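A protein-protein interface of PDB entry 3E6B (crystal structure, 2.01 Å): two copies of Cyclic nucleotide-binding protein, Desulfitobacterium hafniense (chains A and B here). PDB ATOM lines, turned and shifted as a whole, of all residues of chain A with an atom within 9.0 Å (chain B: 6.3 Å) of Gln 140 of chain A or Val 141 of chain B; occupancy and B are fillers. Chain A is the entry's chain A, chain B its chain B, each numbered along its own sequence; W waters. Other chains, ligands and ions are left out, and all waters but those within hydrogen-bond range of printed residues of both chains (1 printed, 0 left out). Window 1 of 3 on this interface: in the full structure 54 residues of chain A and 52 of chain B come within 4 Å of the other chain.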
ATOM      1  N   ASP A  17      28.269  23.383  -2.818  1.00  0.00           N
ATOM      2  CA  ASP A  17      28.401  24.789  -3.316  1.00  0.00           C
ATOM      3  C   ASP A  17      28.967  24.860  -4.777  1.00  0.00           C
ATOM      4  O   ASP A  17      28.952  23.845  -5.504  1.00  0.00           O
ATOM      5  CB  ASP A  17      29.221  25.633  -2.319  1.00  0.00           C
ATOM      6  CG  ASP A  17      28.813  27.112  -2.307  1.00  0.00           C
ATOM      7  OD1 ASP A  17      28.870  27.761  -3.382  1.00  0.00           O
ATOM      8  OD2 ASP A  17      28.446  27.634  -1.220  1.00  0.00           O
ATOM      9  N   PHE A  19      29.405  25.251  -8.638  1.00  0.00           N
ATOM     10  CA  PHE A  19      29.721  24.338  -9.724  1.00  0.00           C
ATOM     11  C   PHE A  19      30.096  25.081 -10.966  1.00  0.00           C
ATOM     12  O   PHE A  19      29.370  26.047 -11.371  1.00  0.00           O
ATOM     13  CB  PHE A  19      28.571  23.395 -10.024  1.00  0.00           C
ATOM     14  CG  PHE A  19      28.598  22.177  -9.203  1.00  0.00           C
ATOM     15  CD1 PHE A  19      29.705  21.337  -9.243  1.00  0.00           C
ATOM     16  CD2 PHE A  19      27.531  21.870  -8.360  1.00  0.00           C
ATOM     17  CE1 PHE A  19      29.744  20.220  -8.480  1.00  0.00           C
ATOM     18  CE2 PHE A  19      27.575  20.740  -7.586  1.00  0.00           C
ATOM     19  CZ  PHE A  19      28.688  19.916  -7.657  1.00  0.00           C
ATOM     20  N   ILE A  65      16.276  18.272  -2.765  1.00  0.00           N
ATOM     21  CA  ILE A  65      15.485  17.157  -3.296  1.00  0.00           C
ATOM     22  C   ILE A  65      14.421  16.801  -2.247  1.00  0.00           C
ATOM     23  O   ILE A  65      14.654  16.916  -1.035  1.00  0.00           O
ATOM     24  CB  ILE A  65      16.343  15.894  -3.656  1.00  0.00           C
ATOM     25  CG1 ILE A  65      17.403  16.210  -4.695  1.00  0.00           C
ATOM     26  CG2 ILE A  65      15.474  14.767  -4.231  1.00  0.00           C
ATOM     27  CD1 ILE A  65      17.998  14.962  -5.371  1.00  0.00           C
ATOM     28  N   PHE A  67      12.110  13.693  -1.192  1.00  0.00           N
ATOM     29  CA  PHE A  67      11.962  12.270  -1.481  1.00  0.00           C
ATOM     30  C   PHE A  67      10.492  11.912  -1.408  1.00  0.00           C
ATOM     31  O   PHE A  67       9.693  12.690  -0.874  1.00  0.00           O
ATOM     32  CB  PHE A  67      12.829  11.452  -0.524  1.00  0.00           C
ATOM     33  CG  PHE A  67      14.291  11.477  -0.888  1.00  0.00           C
ATOM     34  CD1 PHE A  67      14.868  10.401  -1.530  1.00  0.00           C
ATOM     35  CD2 PHE A  67      15.068  12.616  -0.649  1.00  0.00           C
ATOM     36  CE1 PHE A  67      16.221  10.440  -1.896  1.00  0.00           C
ATOM     37  CE2 PHE A  67      16.412  12.664  -1.027  1.00  0.00           C
ATOM     38  CZ  PHE A  67      16.987  11.585  -1.638  1.00  0.00           C
ATOM     39  N   LYS A  73      16.002  17.154   1.545  1.00  0.00           N
ATOM     40  CA  LYS A  73      17.450  17.120   1.699  1.00  0.00           C
ATOM     41  C   LYS A  73      18.151  18.092   0.760  1.00  0.00           C
ATOM     42  O   LYS A  73      17.745  18.291  -0.399  1.00  0.00           O
ATOM     43  CB  LYS A  73      17.903  15.680   1.554  1.00  0.00           C
ATOM     44  CG  LYS A  73      16.952  14.813   2.348  1.00  0.00           C
ATOM     45  CD  LYS A  73      17.267  13.356   2.439  1.00  0.00           C
ATOM     46  CE  LYS A  73      16.623  12.838   3.693  1.00  0.00           C
ATOM     47  NZ  LYS A  73      16.422  11.402   3.576  1.00  0.00           N
ATOM     48  N   LEU A  74      19.170  18.751   1.278  1.00  0.00           N
ATOM     49  CA  LEU A  74      19.938  19.710   0.493  1.00  0.00           C
ATOM     50  C   LEU A  74      20.778  18.958  -0.538  1.00  0.00           C
ATOM     51  O   LEU A  74      21.356  17.887  -0.245  1.00  0.00           O
ATOM     52  CB  LEU A  74      20.812  20.573   1.409  1.00  0.00           C
ATOM     53  CG  LEU A  74      21.935  21.488   0.925  1.00  0.00           C
ATOM     54  CD1 LEU A  74      21.411  22.800   0.380  1.00  0.00           C
ATOM     55  CD2 LEU A  74      22.870  21.749   2.076  1.00  0.00           C
ATOM     56  N   LEU A  75      20.821  19.530  -1.747  1.00  0.00           N
ATOM     57  CA  LEU A  75      21.688  19.063  -2.814  1.00  0.00           C
ATOM     58  C   LEU A  75      22.847  20.049  -2.928  1.00  0.00           C
ATOM     59  O   LEU A  75      24.031  19.689  -2.767  1.00  0.00           O
ATOM     60  CB  LEU A  75      20.906  19.005  -4.126  1.00  0.00           C
ATOM     61  CG  LEU A  75      20.929  17.709  -4.920  1.00  0.00           C
ATOM     62  CD1 LEU A  75      20.540  17.966  -6.381  1.00  0.00           C
ATOM     63  CD2 LEU A  75      22.312  17.084  -4.826  1.00  0.00           C
ATOM     64  N   TYR A  76      22.520  21.300  -3.213  1.00  0.00           N
ATOM     65  CA  TYR A  76      23.571  22.288  -3.246  1.00  0.00           C
ATOM     66  C   TYR A  76      23.077  23.702  -3.049  1.00  0.00           C
ATOM     67  O   TYR A  76      21.894  23.978  -3.158  1.00  0.00           O
ATOM     68  CB  TYR A  76      24.420  22.189  -4.523  1.00  0.00           C
ATOM     69  CG  TYR A  76      23.735  22.481  -5.867  1.00  0.00           C
ATOM     70  CD1 TYR A  76      23.478  21.449  -6.792  1.00  0.00           C
ATOM     71  CD2 TYR A  76      23.380  23.789  -6.233  1.00  0.00           C
ATOM     72  CE1 TYR A  76      22.890  21.724  -8.072  1.00  0.00           C
ATOM     73  CE2 TYR A  76      22.784  24.070  -7.493  1.00  0.00           C
ATOM     74  CZ  TYR A  76      22.559  23.032  -8.408  1.00  0.00           C
ATOM     75  OH  TYR A  76      21.975  23.332  -9.618  1.00  0.00           O
ATOM     76  N   LYS A 133      29.876  18.412 -12.097  1.00  0.00           N
ATOM     77  CA  LYS A 133      28.859  17.884 -11.199  1.00  0.00           C
ATOM     78  C   LYS A 133      28.886  16.344 -11.111  1.00  0.00           C
ATOM     79  O   LYS A 133      28.703  15.793 -10.007  1.00  0.00           O
ATOM     80  CB  LYS A 133      27.467  18.367 -11.644  1.00  0.00           C
ATOM     81  CG  LYS A 133      27.230  19.853 -11.462  1.00  0.00           C
ATOM     82  CD  LYS A 133      25.802  20.258 -12.088  1.00  0.00           C
ATOM     83  CE  LYS A 133      25.551  21.775 -12.038  1.00  0.00           C
ATOM     84  NZ  LYS A 133      24.224  22.068 -12.727  1.00  0.00           N
ATOM     85  N   VAL A 134      29.058  15.629 -12.236  1.00  0.00           N
ATOM     86  CA  VAL A 134      29.072  14.136 -12.207  1.00  0.00           C
ATOM     87  C   VAL A 134      30.321  13.673 -11.391  1.00  0.00           C
ATOM     88  O   VAL A 134      30.220  12.754 -10.546  1.00  0.00           O
ATOM     89  CB  VAL A 134      29.104  13.456 -13.650  1.00  0.00           C
ATOM     90  CG1 VAL A 134      29.189  11.961 -13.549  1.00  0.00           C
ATOM     91  CG2 VAL A 134      27.798  13.809 -14.496  1.00  0.00           C
ATOM     92  N   ALA A 135      31.452  14.350 -11.632  1.00  0.00           N
ATOM     93  CA  ALA A 135      32.750  14.046 -11.030  1.00  0.00           C
ATOM     94  C   ALA A 135      32.596  14.243  -9.530  1.00  0.00           C
ATOM     95  O   ALA A 135      32.887  13.344  -8.765  1.00  0.00           O
ATOM     96  CB  ALA A 135      33.853  14.963 -11.584  1.00  0.00           C
ATOM     97  N   TYR A 136      32.109  15.401  -9.145  1.00  0.00           N
ATOM     98  CA  TYR A 136      31.780  15.707  -7.740  1.00  0.00           C
ATOM     99  C   TYR A 136      30.862  14.717  -7.002  1.00  0.00           C
ATOM    100  O   TYR A 136      31.283  14.131  -6.011  1.00  0.00           O
ATOM    101  CB  TYR A 136      31.242  17.123  -7.591  1.00  0.00           C
ATOM    102  CG  TYR A 136      30.969  17.463  -6.146  1.00  0.00           C
ATOM    103  CD1 TYR A 136      31.976  17.945  -5.314  1.00  0.00           C
ATOM    104  CD2 TYR A 136      29.697  17.265  -5.608  1.00  0.00           C
ATOM    105  CE1 TYR A 136      31.706  18.269  -3.975  1.00  0.00           C
ATOM    106  CE2 TYR A 136      29.420  17.550  -4.286  1.00  0.00           C
ATOM    107  CZ  TYR A 136      30.415  18.067  -3.484  1.00  0.00           C
ATOM    108  OH  TYR A 136      30.087  18.343  -2.160  1.00  0.00           O
ATOM    109  N   TYR A 137      29.628  14.555  -7.443  1.00  0.00           N
ATOM    110  CA  TYR A 137      28.701  13.625  -6.795  1.00  0.00           C
ATOM    111  C   TYR A 137      29.120  12.141  -6.867  1.00  0.00           C
ATOM    112  O   TYR A 137      29.041  11.438  -5.870  1.00  0.00           O
ATOM    113  CB  TYR A 137      27.258  13.847  -7.276  1.00  0.00           C
ATOM    114  CG  TYR A 137      26.692  15.178  -6.829  1.00  0.00           C
ATOM    115  CD1 TYR A 137      26.424  15.424  -5.483  1.00  0.00           C
ATOM    116  CD2 TYR A 137      26.465  16.210  -7.750  1.00  0.00           C
ATOM    117  CE1 TYR A 137      25.902  16.647  -5.069  1.00  0.00           C
ATOM    118  CE2 TYR A 137      25.986  17.430  -7.347  1.00  0.00           C
ATOM    119  CZ  TYR A 137      25.687  17.643  -6.001  1.00  0.00           C
ATOM    120  OH  TYR A 137      25.197  18.875  -5.597  1.00  0.00           O
ATOM    121  N   ALA A 138      29.577  11.665  -8.024  1.00  0.00           N
ATOM    122  CA  ALA A 138      30.049  10.290  -8.144  1.00  0.00           C
ATOM    123  C   ALA A 138      31.169   9.951  -7.176  1.00  0.00           C
ATOM    124  O   ALA A 138      31.247   8.830  -6.713  1.00  0.00           O
ATOM    125  CB  ALA A 138      30.490   9.985  -9.553  1.00  0.00           C
ATOM    126  N   ARG A 139      32.063  10.909  -6.938  1.00  0.00           N
ATOM    127  CA  ARG A 139      33.224  10.683  -6.094  1.00  0.00           C
ATOM    128  C   ARG A 139      32.730  10.571  -4.647  1.00  0.00           C
ATOM    129  O   ARG A 139      33.220   9.756  -3.879  1.00  0.00           O
ATOM    130  CB  ARG A 139      34.224  11.832  -6.215  1.00  0.00           C
ATOM    131  CG  ARG A 139      35.405  11.683  -5.268  1.00  0.00           C
ATOM    132  CD  ARG A 139      36.416  12.785  -5.447  1.00  0.00           C
ATOM    133  NE  ARG A 139      37.573  12.607  -4.563  1.00  0.00           N
ATOM    134  CZ  ARG A 139      38.678  11.918  -4.841  1.00  0.00           C
ATOM    135  NH1 ARG A 139      38.844  11.289  -6.008  1.00  0.00           N
ATOM    136  NH2 ARG A 139      39.632  11.840  -3.924  1.00  0.00           N
ATOM    137  N   GLN A 140      31.749  11.393  -4.289  1.00  0.00           N
ATOM    138  CA  GLN A 140      31.179  11.355  -2.938  1.00  0.00           C
ATOM    139  C   GLN A 140      30.422  10.078  -2.639  1.00  0.00           C
ATOM    140  O   GLN A 140      30.489   9.571  -1.525  1.00  0.00           O
ATOM    141  CB  GLN A 140      30.296  12.546  -2.699  1.00  0.00           C
ATOM    142  CG  GLN A 140      31.088  13.783  -2.566  1.00  0.00           C
ATOM    143  CD  GLN A 140      30.304  14.803  -1.878  1.00  0.00           C
ATOM    144  OE1 GLN A 140      29.160  14.548  -1.501  1.00  0.00           O
ATOM    145  NE2 GLN A 140      30.897  15.957  -1.645  1.00  0.00           N
ATOM    146  N   VAL A 141      29.709   9.560  -3.628  1.00  0.00           N
ATOM    147  CA  VAL A 141      29.015   8.300  -3.446  1.00  0.00           C
ATOM    148  C   VAL A 141      30.084   7.255  -3.140  1.00  0.00           C
ATOM    149  O   VAL A 141      29.914   6.432  -2.234  1.00  0.00           O
ATOM    150  CB  VAL A 141      28.150   7.912  -4.690  1.00  0.00           C
ATOM    151  CG1 VAL A 141      27.635   6.464  -4.601  1.00  0.00           C
ATOM    152  CG2 VAL A 141      26.980   8.897  -4.865  1.00  0.00           C
ATOM    153  N   ALA A 142      31.188   7.310  -3.891  1.00  0.00           N
ATOM    154  CA  ALA A 142      32.257   6.320  -3.787  1.00  0.00           C
ATOM    155  C   ALA A 142      32.979   6.418  -2.437  1.00  0.00           C
ATOM    156  O   ALA A 142      33.186   5.394  -1.771  1.00  0.00           O
ATOM    157  CB  ALA A 142      33.250   6.462  -4.956  1.00  0.00           C
ATOM    158  N   GLU A 143      33.326   7.646  -2.037  1.00  0.00           N
ATOM    159  CA  GLU A 143      34.031   7.895  -0.789  1.00  0.00           C
ATOM    160  C   GLU A 143      33.280   7.269   0.382  1.00  0.00           C
ATOM    161  O   GLU A 143      33.881   6.679   1.272  1.00  0.00           O
ATOM    162  CB  GLU A 143      34.216   9.380  -0.554  1.00  0.00           C
ATOM    163  CG  GLU A 143      35.291   9.997  -1.405  1.00  0.00           C
ATOM    164  CD  GLU A 143      35.542  11.458  -1.063  1.00  0.00           C
ATOM    165  OE1 GLU A 143      36.522  12.050  -1.586  1.00  0.00           O
ATOM    166  OE2 GLU A 143      34.759  12.023  -0.274  1.00  0.00           O
ATOM    167  N   MET A 144      31.958   7.379   0.351  1.00  0.00           N
ATOM    168  CA  MET A 144      31.086   6.700   1.296  1.00  0.00           C
ATOM    169  C   MET A 144      30.650   5.364   0.720  1.00  0.00           C
ATOM    170  O   MET A 144      31.119   4.316   1.148  1.00  0.00           O
ATOM    171  CB  MET A 144      29.872   7.570   1.549  1.00  0.00           C
ATOM    172  CG  MET A 144      30.230   9.052   1.562  1.00  0.00           C
ATOM    173  SD  MET A 144      28.778  10.103   1.743  1.00  0.00           S
ATOM    174  CE  MET A 144      28.624  10.211   3.552  1.00  0.00           C
ATOM    175  N   GLY A 188      23.495   6.297   8.152  1.00  0.00           N
ATOM    176  CA  GLY A 188      24.044   6.906   6.945  1.00  0.00           C
ATOM    177  C   GLY A 188      24.491   5.855   5.948  1.00  0.00           C
ATOM    178  O   GLY A 188      25.480   6.046   5.219  1.00  0.00           O
ATOM    179  N   HIS A 190      23.547   3.473   2.702  1.00  0.00           N
ATOM    180  CA  HIS A 190      22.643   3.471   1.565  1.00  0.00           C
ATOM    181  C   HIS A 190      21.604   2.327   1.720  1.00  0.00           C
ATOM    182  O   HIS A 190      21.943   1.227   2.182  1.00  0.00           O
ATOM    183  CB  HIS A 190      23.442   3.341   0.261  1.00  0.00           C
ATOM    184  CG  HIS A 190      22.599   3.476  -0.969  1.00  0.00           C
ATOM    185  ND1 HIS A 190      22.567   2.519  -1.959  1.00  0.00           N
ATOM    186  CD2 HIS A 190      21.714   4.436  -1.345  1.00  0.00           C
ATOM    187  CE1 HIS A 190      21.719   2.895  -2.904  1.00  0.00           C
ATOM    188  NE2 HIS A 190      21.172   4.043  -2.546  1.00  0.00           N
ATOM    189  N   TYR B 136      21.140  10.820 -10.868  1.00  0.00           N
ATOM    190  CA  TYR B 136      21.419   9.553 -10.178  1.00  0.00           C
ATOM    191  C   TYR B 136      22.378   9.651  -8.968  1.00  0.00           C
ATOM    192  O   TYR B 136      22.061   9.140  -7.871  1.00  0.00           O
ATOM    193  CB  TYR B 136      21.924   8.499 -11.182  1.00  0.00           C
ATOM    194  CG  TYR B 136      22.268   7.218 -10.507  1.00  0.00           C
ATOM    195  CD1 TYR B 136      21.302   6.256 -10.298  1.00  0.00           C
ATOM    196  CD2 TYR B 136      23.559   6.958 -10.071  1.00  0.00           C
ATOM    197  CE1 TYR B 136      21.609   5.065  -9.654  1.00  0.00           C
ATOM    198  CE2 TYR B 136      23.869   5.773  -9.415  1.00  0.00           C
ATOM    199  CZ  TYR B 136      22.875   4.843  -9.220  1.00  0.00           C
ATOM    200  OH  TYR B 136      23.141   3.664  -8.591  1.00  0.00           O
ATOM    201  N   TYR B 137      23.534  10.301  -9.149  1.00  0.00           N
ATOM    202  CA  TYR B 137      24.481  10.429  -8.076  1.00  0.00           C
ATOM    203  C   TYR B 137      24.106  11.401  -7.007  1.00  0.00           C
ATOM    204  O   TYR B 137      24.403  11.150  -5.840  1.00  0.00           O
ATOM    205  CB  TYR B 137      25.922  10.718  -8.574  1.00  0.00           C
ATOM    206  CG  TYR B 137      26.471   9.603  -9.391  1.00  0.00           C
ATOM    207  CD1 TYR B 137      26.900   8.401  -8.772  1.00  0.00           C
ATOM    208  CD2 TYR B 137      26.545   9.709 -10.782  1.00  0.00           C
ATOM    209  CE1 TYR B 137      27.417   7.343  -9.526  1.00  0.00           C
ATOM    210  CE2 TYR B 137      27.070   8.652 -11.552  1.00  0.00           C
ATOM    211  CZ  TYR B 137      27.483   7.477 -10.933  1.00  0.00           C
ATOM    212  OH  TYR B 137      27.988   6.458 -11.699  1.00  0.00           O
ATOM    213  N   ALA B 138      23.480  12.513  -7.399  1.00  0.00           N
ATOM    214  CA  ALA B 138      23.014  13.527  -6.460  1.00  0.00           C
ATOM    215  C   ALA B 138      21.902  13.009  -5.544  1.00  0.00           C
ATOM    216  O   ALA B 138      21.869  13.393  -4.372  1.00  0.00           O
ATOM    217  CB  ALA B 138      22.540  14.760  -7.191  1.00  0.00           C
ATOM    218  N   ARG B 139      20.984  12.192  -6.071  1.00  0.00           N
ATOM    219  CA  ARG B 139      19.930  11.639  -5.256  1.00  0.00           C
ATOM    220  C   ARG B 139      20.508  10.731  -4.156  1.00  0.00           C
ATOM    221  O   ARG B 139      20.024  10.760  -3.021  1.00  0.00           O
ATOM    222  CB  ARG B 139      18.962  10.831  -6.092  1.00  0.00           C
ATOM    223  CG  ARG B 139      17.770  10.250  -5.318  1.00  0.00           C
ATOM    224  CD  ARG B 139      16.983   9.389  -6.277  1.00  0.00           C
ATOM    225  NE  ARG B 139      15.739   8.858  -5.708  1.00  0.00           N
ATOM    226  CZ  ARG B 139      14.625   9.554  -5.485  1.00  0.00           C
ATOM    227  NH1 ARG B 139      14.554  10.854  -5.758  1.00  0.00           N
ATOM    228  NH2 ARG B 139      13.569   8.940  -4.955  1.00  0.00           N
ATOM    229  N   GLN B 140      21.490   9.905  -4.512  1.00  0.00           N
ATOM    230  CA  GLN B 140      22.218   9.009  -3.533  1.00  0.00           C
ATOM    231  C   GLN B 140      22.947   9.814  -2.406  1.00  0.00           C
ATOM    232  O   GLN B 140      22.839   9.484  -1.189  1.00  0.00           O
ATOM    233  CB  GLN B 140      23.208   8.069  -4.238  1.00  0.00           C
ATOM    234  CG  GLN B 140      22.742   7.129  -5.419  1.00  0.00           C
ATOM    235  CD  GLN B 140      21.248   6.695  -5.444  1.00  0.00           C
ATOM    236  OE1 GLN B 140      20.548   6.841  -6.475  1.00  0.00           O
ATOM    237  NE2 GLN B 140      20.763   6.159  -4.330  1.00  0.00           N
ATOM    238  N   VAL B 141      23.657  10.884  -2.796  1.00  0.00           N
ATOM    239  CA  VAL B 141      24.328  11.760  -1.842  1.00  0.00           C
ATOM    240  C   VAL B 141      23.285  12.365  -0.902  1.00  0.00           C
ATOM    241  O   VAL B 141      23.486  12.353   0.321  1.00  0.00           O
ATOM    242  CB  VAL B 141      25.122  12.879  -2.550  1.00  0.00           C
ATOM    243  CG1 VAL B 141      25.551  13.992  -1.583  1.00  0.00           C
ATOM    244  CG2 VAL B 141      26.331  12.318  -3.186  1.00  0.00           C
ATOM    245  N   ALA B 142      22.166  12.850  -1.469  1.00  0.00           N
ATOM    246  CA  ALA B 142      21.093  13.477  -0.700  1.00  0.00           C
ATOM    247  C   ALA B 142      20.417  12.519   0.265  1.00  0.00           C
ATOM    248  O   ALA B 142      20.027  12.925   1.371  1.00  0.00           O
ATOM    249  CB  ALA B 142      20.003  14.139  -1.637  1.00  0.00           C
ATOM    250  N   GLU B 143      20.219  11.279  -0.158  1.00  0.00           N
ATOM    251  CA  GLU B 143      19.514  10.300   0.659  1.00  0.00           C
ATOM    252  C   GLU B 143      20.284  10.100   1.971  1.00  0.00           C
ATOM    253  O   GLU B 143      19.705  10.071   3.034  1.00  0.00           O
ATOM    254  CB  GLU B 143      19.360   8.959  -0.096  1.00  0.00           C
ATOM    255  CG  GLU B 143      19.211   7.753   0.851  1.00  0.00           C
ATOM    256  CD  GLU B 143      19.154   6.392   0.152  1.00  0.00           C
ATOM    257  OE1 GLU B 143      18.863   6.331  -1.088  1.00  0.00           O
ATOM    258  OE2 GLU B 143      19.393   5.375   0.858  1.00  0.00           O
ATOM    259  N   MET B 144      21.599  10.025   1.891  1.00  0.00           N
ATOM    260  CA  MET B 144      22.398   9.704   3.042  1.00  0.00           C
ATOM    261  C   MET B 144      22.719  10.849   4.034  1.00  0.00           C
ATOM    262  O   MET B 144      23.583  10.673   4.901  1.00  0.00           O
ATOM    263  CB  MET B 144      23.657   8.992   2.594  1.00  0.00           C
ATOM    264  CG  MET B 144      23.423   7.516   2.244  1.00  0.00           C
ATOM    265  SD  MET B 144      24.748   7.264   1.073  1.00  0.00           S
ATOM    266  CE  MET B 144      26.302   7.153   1.951  1.00  0.00           C
ATOM    267  N   ASN B 145      22.017  11.978   3.888  1.00  0.00           N
ATOM    268  CA  ASN B 145      22.140  13.173   4.764  1.00  0.00           C
ATOM    269  C   ASN B 145      23.576  13.670   4.889  1.00  0.00           C
ATOM    270  O   ASN B 145      24.018  14.149   5.950  1.00  0.00           O
ATOM    271  CB  ASN B 145      21.513  12.908   6.159  1.00  0.00           C
ATOM    272  CG  ASN B 145      20.040  12.668   6.075  1.00  0.00           C
ATOM    273  OD1 ASN B 145      19.557  11.555   6.354  1.00  0.00           O
ATOM    274  ND2 ASN B 145      19.305  13.682   5.674  1.00  0.00           N
ATOM    275  N   THR B 146      24.298  13.569   3.775  1.00  0.00           N
ATOM    276  CA  THR B 146      25.715  13.868   3.730  1.00  0.00           C
ATOM    277  C   THR B 146      25.995  15.261   4.249  1.00  0.00           C
ATOM    278  O   THR B 146      27.020  15.462   4.877  1.00  0.00           O
ATOM    279  CB  THR B 146      26.255  13.789   2.265  1.00  0.00           C
ATOM    280  OG1 THR B 146      25.934  12.509   1.717  1.00  0.00           O
ATOM    281  CG2 THR B 146      27.742  14.032   2.238  1.00  0.00           C
ATOM    282  N   TYR B 147      25.096  16.212   3.995  1.00  0.00           N
ATOM    283  CA  TYR B 147      25.338  17.611   4.356  1.00  0.00           C
ATOM    284  C   TYR B 147      24.658  18.071   5.691  1.00  0.00           C
ATOM    285  O   TYR B 147      25.002  19.141   6.220  1.00  0.00           O
ATOM    286  CB  TYR B 147      24.956  18.550   3.167  1.00  0.00           C
ATOM    287  CG  TYR B 147      25.601  18.153   1.832  1.00  0.00           C
ATOM    288  CD1 TYR B 147      24.844  18.023   0.651  1.00  0.00           C
ATOM    289  CD2 TYR B 147      26.976  17.876   1.764  1.00  0.00           C
ATOM    290  CE1 TYR B 147      25.471  17.615  -0.592  1.00  0.00           C
ATOM    291  CE2 TYR B 147      27.604  17.473   0.552  1.00  0.00           C
ATOM    292  CZ  TYR B 147      26.848  17.357  -0.613  1.00  0.00           C
ATOM    293  OH  TYR B 147      27.518  16.975  -1.776  1.00  0.00           O
HETATM  294  O   HOH W   1      22.094  16.429   2.567  1.00  0.00           O
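The side-chain sulfur of Met 144 of chain A is in hydrogen-bond range of the side-chain hydroxyl of Thr 146 of chain B.
The side-chain hydroxyl of Tyr 136 of chain A sits at hydrogen-bond distance from the side-chain hydroxyl of Tyr 147 of chain B, at 2.9 Å.
A ring nitrogen (NE2) of His 190 of chain A is in hydrogen-bond range of the side-chain amide nitrogen (NE2) of Gln 140 of chain B (2.8 Å).
The side-chain amide oxygen (OE1) of Gln 140 of chain A is in hydrogen-bond range of the side-chain hydroxyl (OH) of Tyr 147 of chain B, at 2.9 Å.
The backbone NH (N) of Ile 65 of chain A lies within hydrogen-bond range of the backbone carbonyl oxygen (O) of Lys 73 of chain A, 2.8 Å away.
The side-chain hydroxyl of Tyr 137 of chain A lies within hydrogen-bond range of the backbone carbonyl oxygen of Leu 75 of chain A, at 3.2 Å.
O of Val 141 of chain B lies within hydrogen-bond range of OG1 of Thr 146 of chain B, 2.8 Å away.
NE2 of Gln 140 of chain A is in hydrogen-bond range of OH of Tyr 136 of chain A.
OE1 of Gln 140 of chain B sits close to O of Tyr 136 of chain B (3.1 Å).
Ala 142 of chain B touches Phe 67 of chain A (CB to CE2, 3.9 Å).
CZ of Phe 67 of chain A touches N of Glu 143 of chain B (3.6 Å).
Tyr 147 of chain B touches Leu 74 of chain A.
Tyr 147 of chain B touches Leu 75 of chain A.
CB of Tyr 137 of chain B touches CB of Tyr 137 of chain A, 3.6 Å away.
Val 141 of chain B touches Tyr 137 of chain A (CG2 to CD1, 3.9 Å).
Val 141 of chain A touches Tyr 137 of chain B (CG2 to O, 3.6 Å).
Val 141 of chain A touches Gln 140 of chain B.
Val 141 of chain A touches Val 141 of chain B.
CB of Met 144 of chain A touches CE of Met 144 of chain B, at 3.6 Å.
Asp 17 of chain A touches none of the printed residues of chain B.
Of the printed residues of chain B, Leu 74 of chain A touches Tyr 147.
Tyr 76 of chain A touches none of the printed residues of chain B.
Of the printed residues of chain B, Ala 138 of chain A touches Tyr 137 (3.7 Å).
Of chain B, only Val 141 (3.7 Å) and Tyr 147 (2.9 Å) come within 4 Å of Gln 140 of chain A.
Val 141 of chain B touches three residues of chain A.
Of chain A, only Phe 67 (3.9 Å) and Lys 73 (3.0 Å) come within 4 Å of Ala 142 of chain B.
The nearest residue of chain B that does not touch Gln 140 of chain A is Thr 146 of chain B (4.03 Å).
Printed residues of chain A that touch a printed residue of chain B: Ile 65, Phe 67, Lys 73, Leu 74, Leu 75, Tyr 136, Tyr 137, Ala 138, Gln 140, Val 141, Met 144, Gly 188 and His 190.
Hydrophobic or aromatic side chains of chain A within 4 Å of the printed part of chain B: Ile 65, Phe 67, Leu 74, Leu 75, Tyr 136, Tyr 137, Val 141, Met 144 and His 190.
Printed residues of chain B that touch a printed residue of chain A: Tyr 137, Ala 138, Arg 139, Gln 140, Val 141, Ala 142, Glu 143, Met 144, Asn 145, Thr 146 and Tyr 147.
Hydrophobic or aromatic side chains of chain B within 4 Å of the printed part of chain A: Tyr 137, Ala 138, Val 141, Ala 142, Met 144 and Tyr 147.
Tyr 137 of chain A touches Val 141 of chain B, and with the chains exchanged Val 141 of chain A touches Tyr 137 of chain B.
Ala 138 of chain A touches Tyr 137 of chain B, but with the chains exchanged Tyr 137 of chain A does not touch Ala 138 of chain B (4.01 Å).
Gln 140 of chain A touches Val 141 of chain B, and with the chains exchanged Val 141 of chain A touches Gln 140 of chain B.
Val 141 of chain B touches its own counterpart, Val 141 of chain A.
Positions printed for both chains: 136, 137, 138, 139, 140, 141, 142, 143 and 144.
Of the 25 pairs that touch across the chains among the printed residues, 7 have their exchanged pair printed and touching as well.
Water W1 bridges O of Leu 74 of chain A (3.3 Å) and N of Tyr 147 of chain B (3.3 Å).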
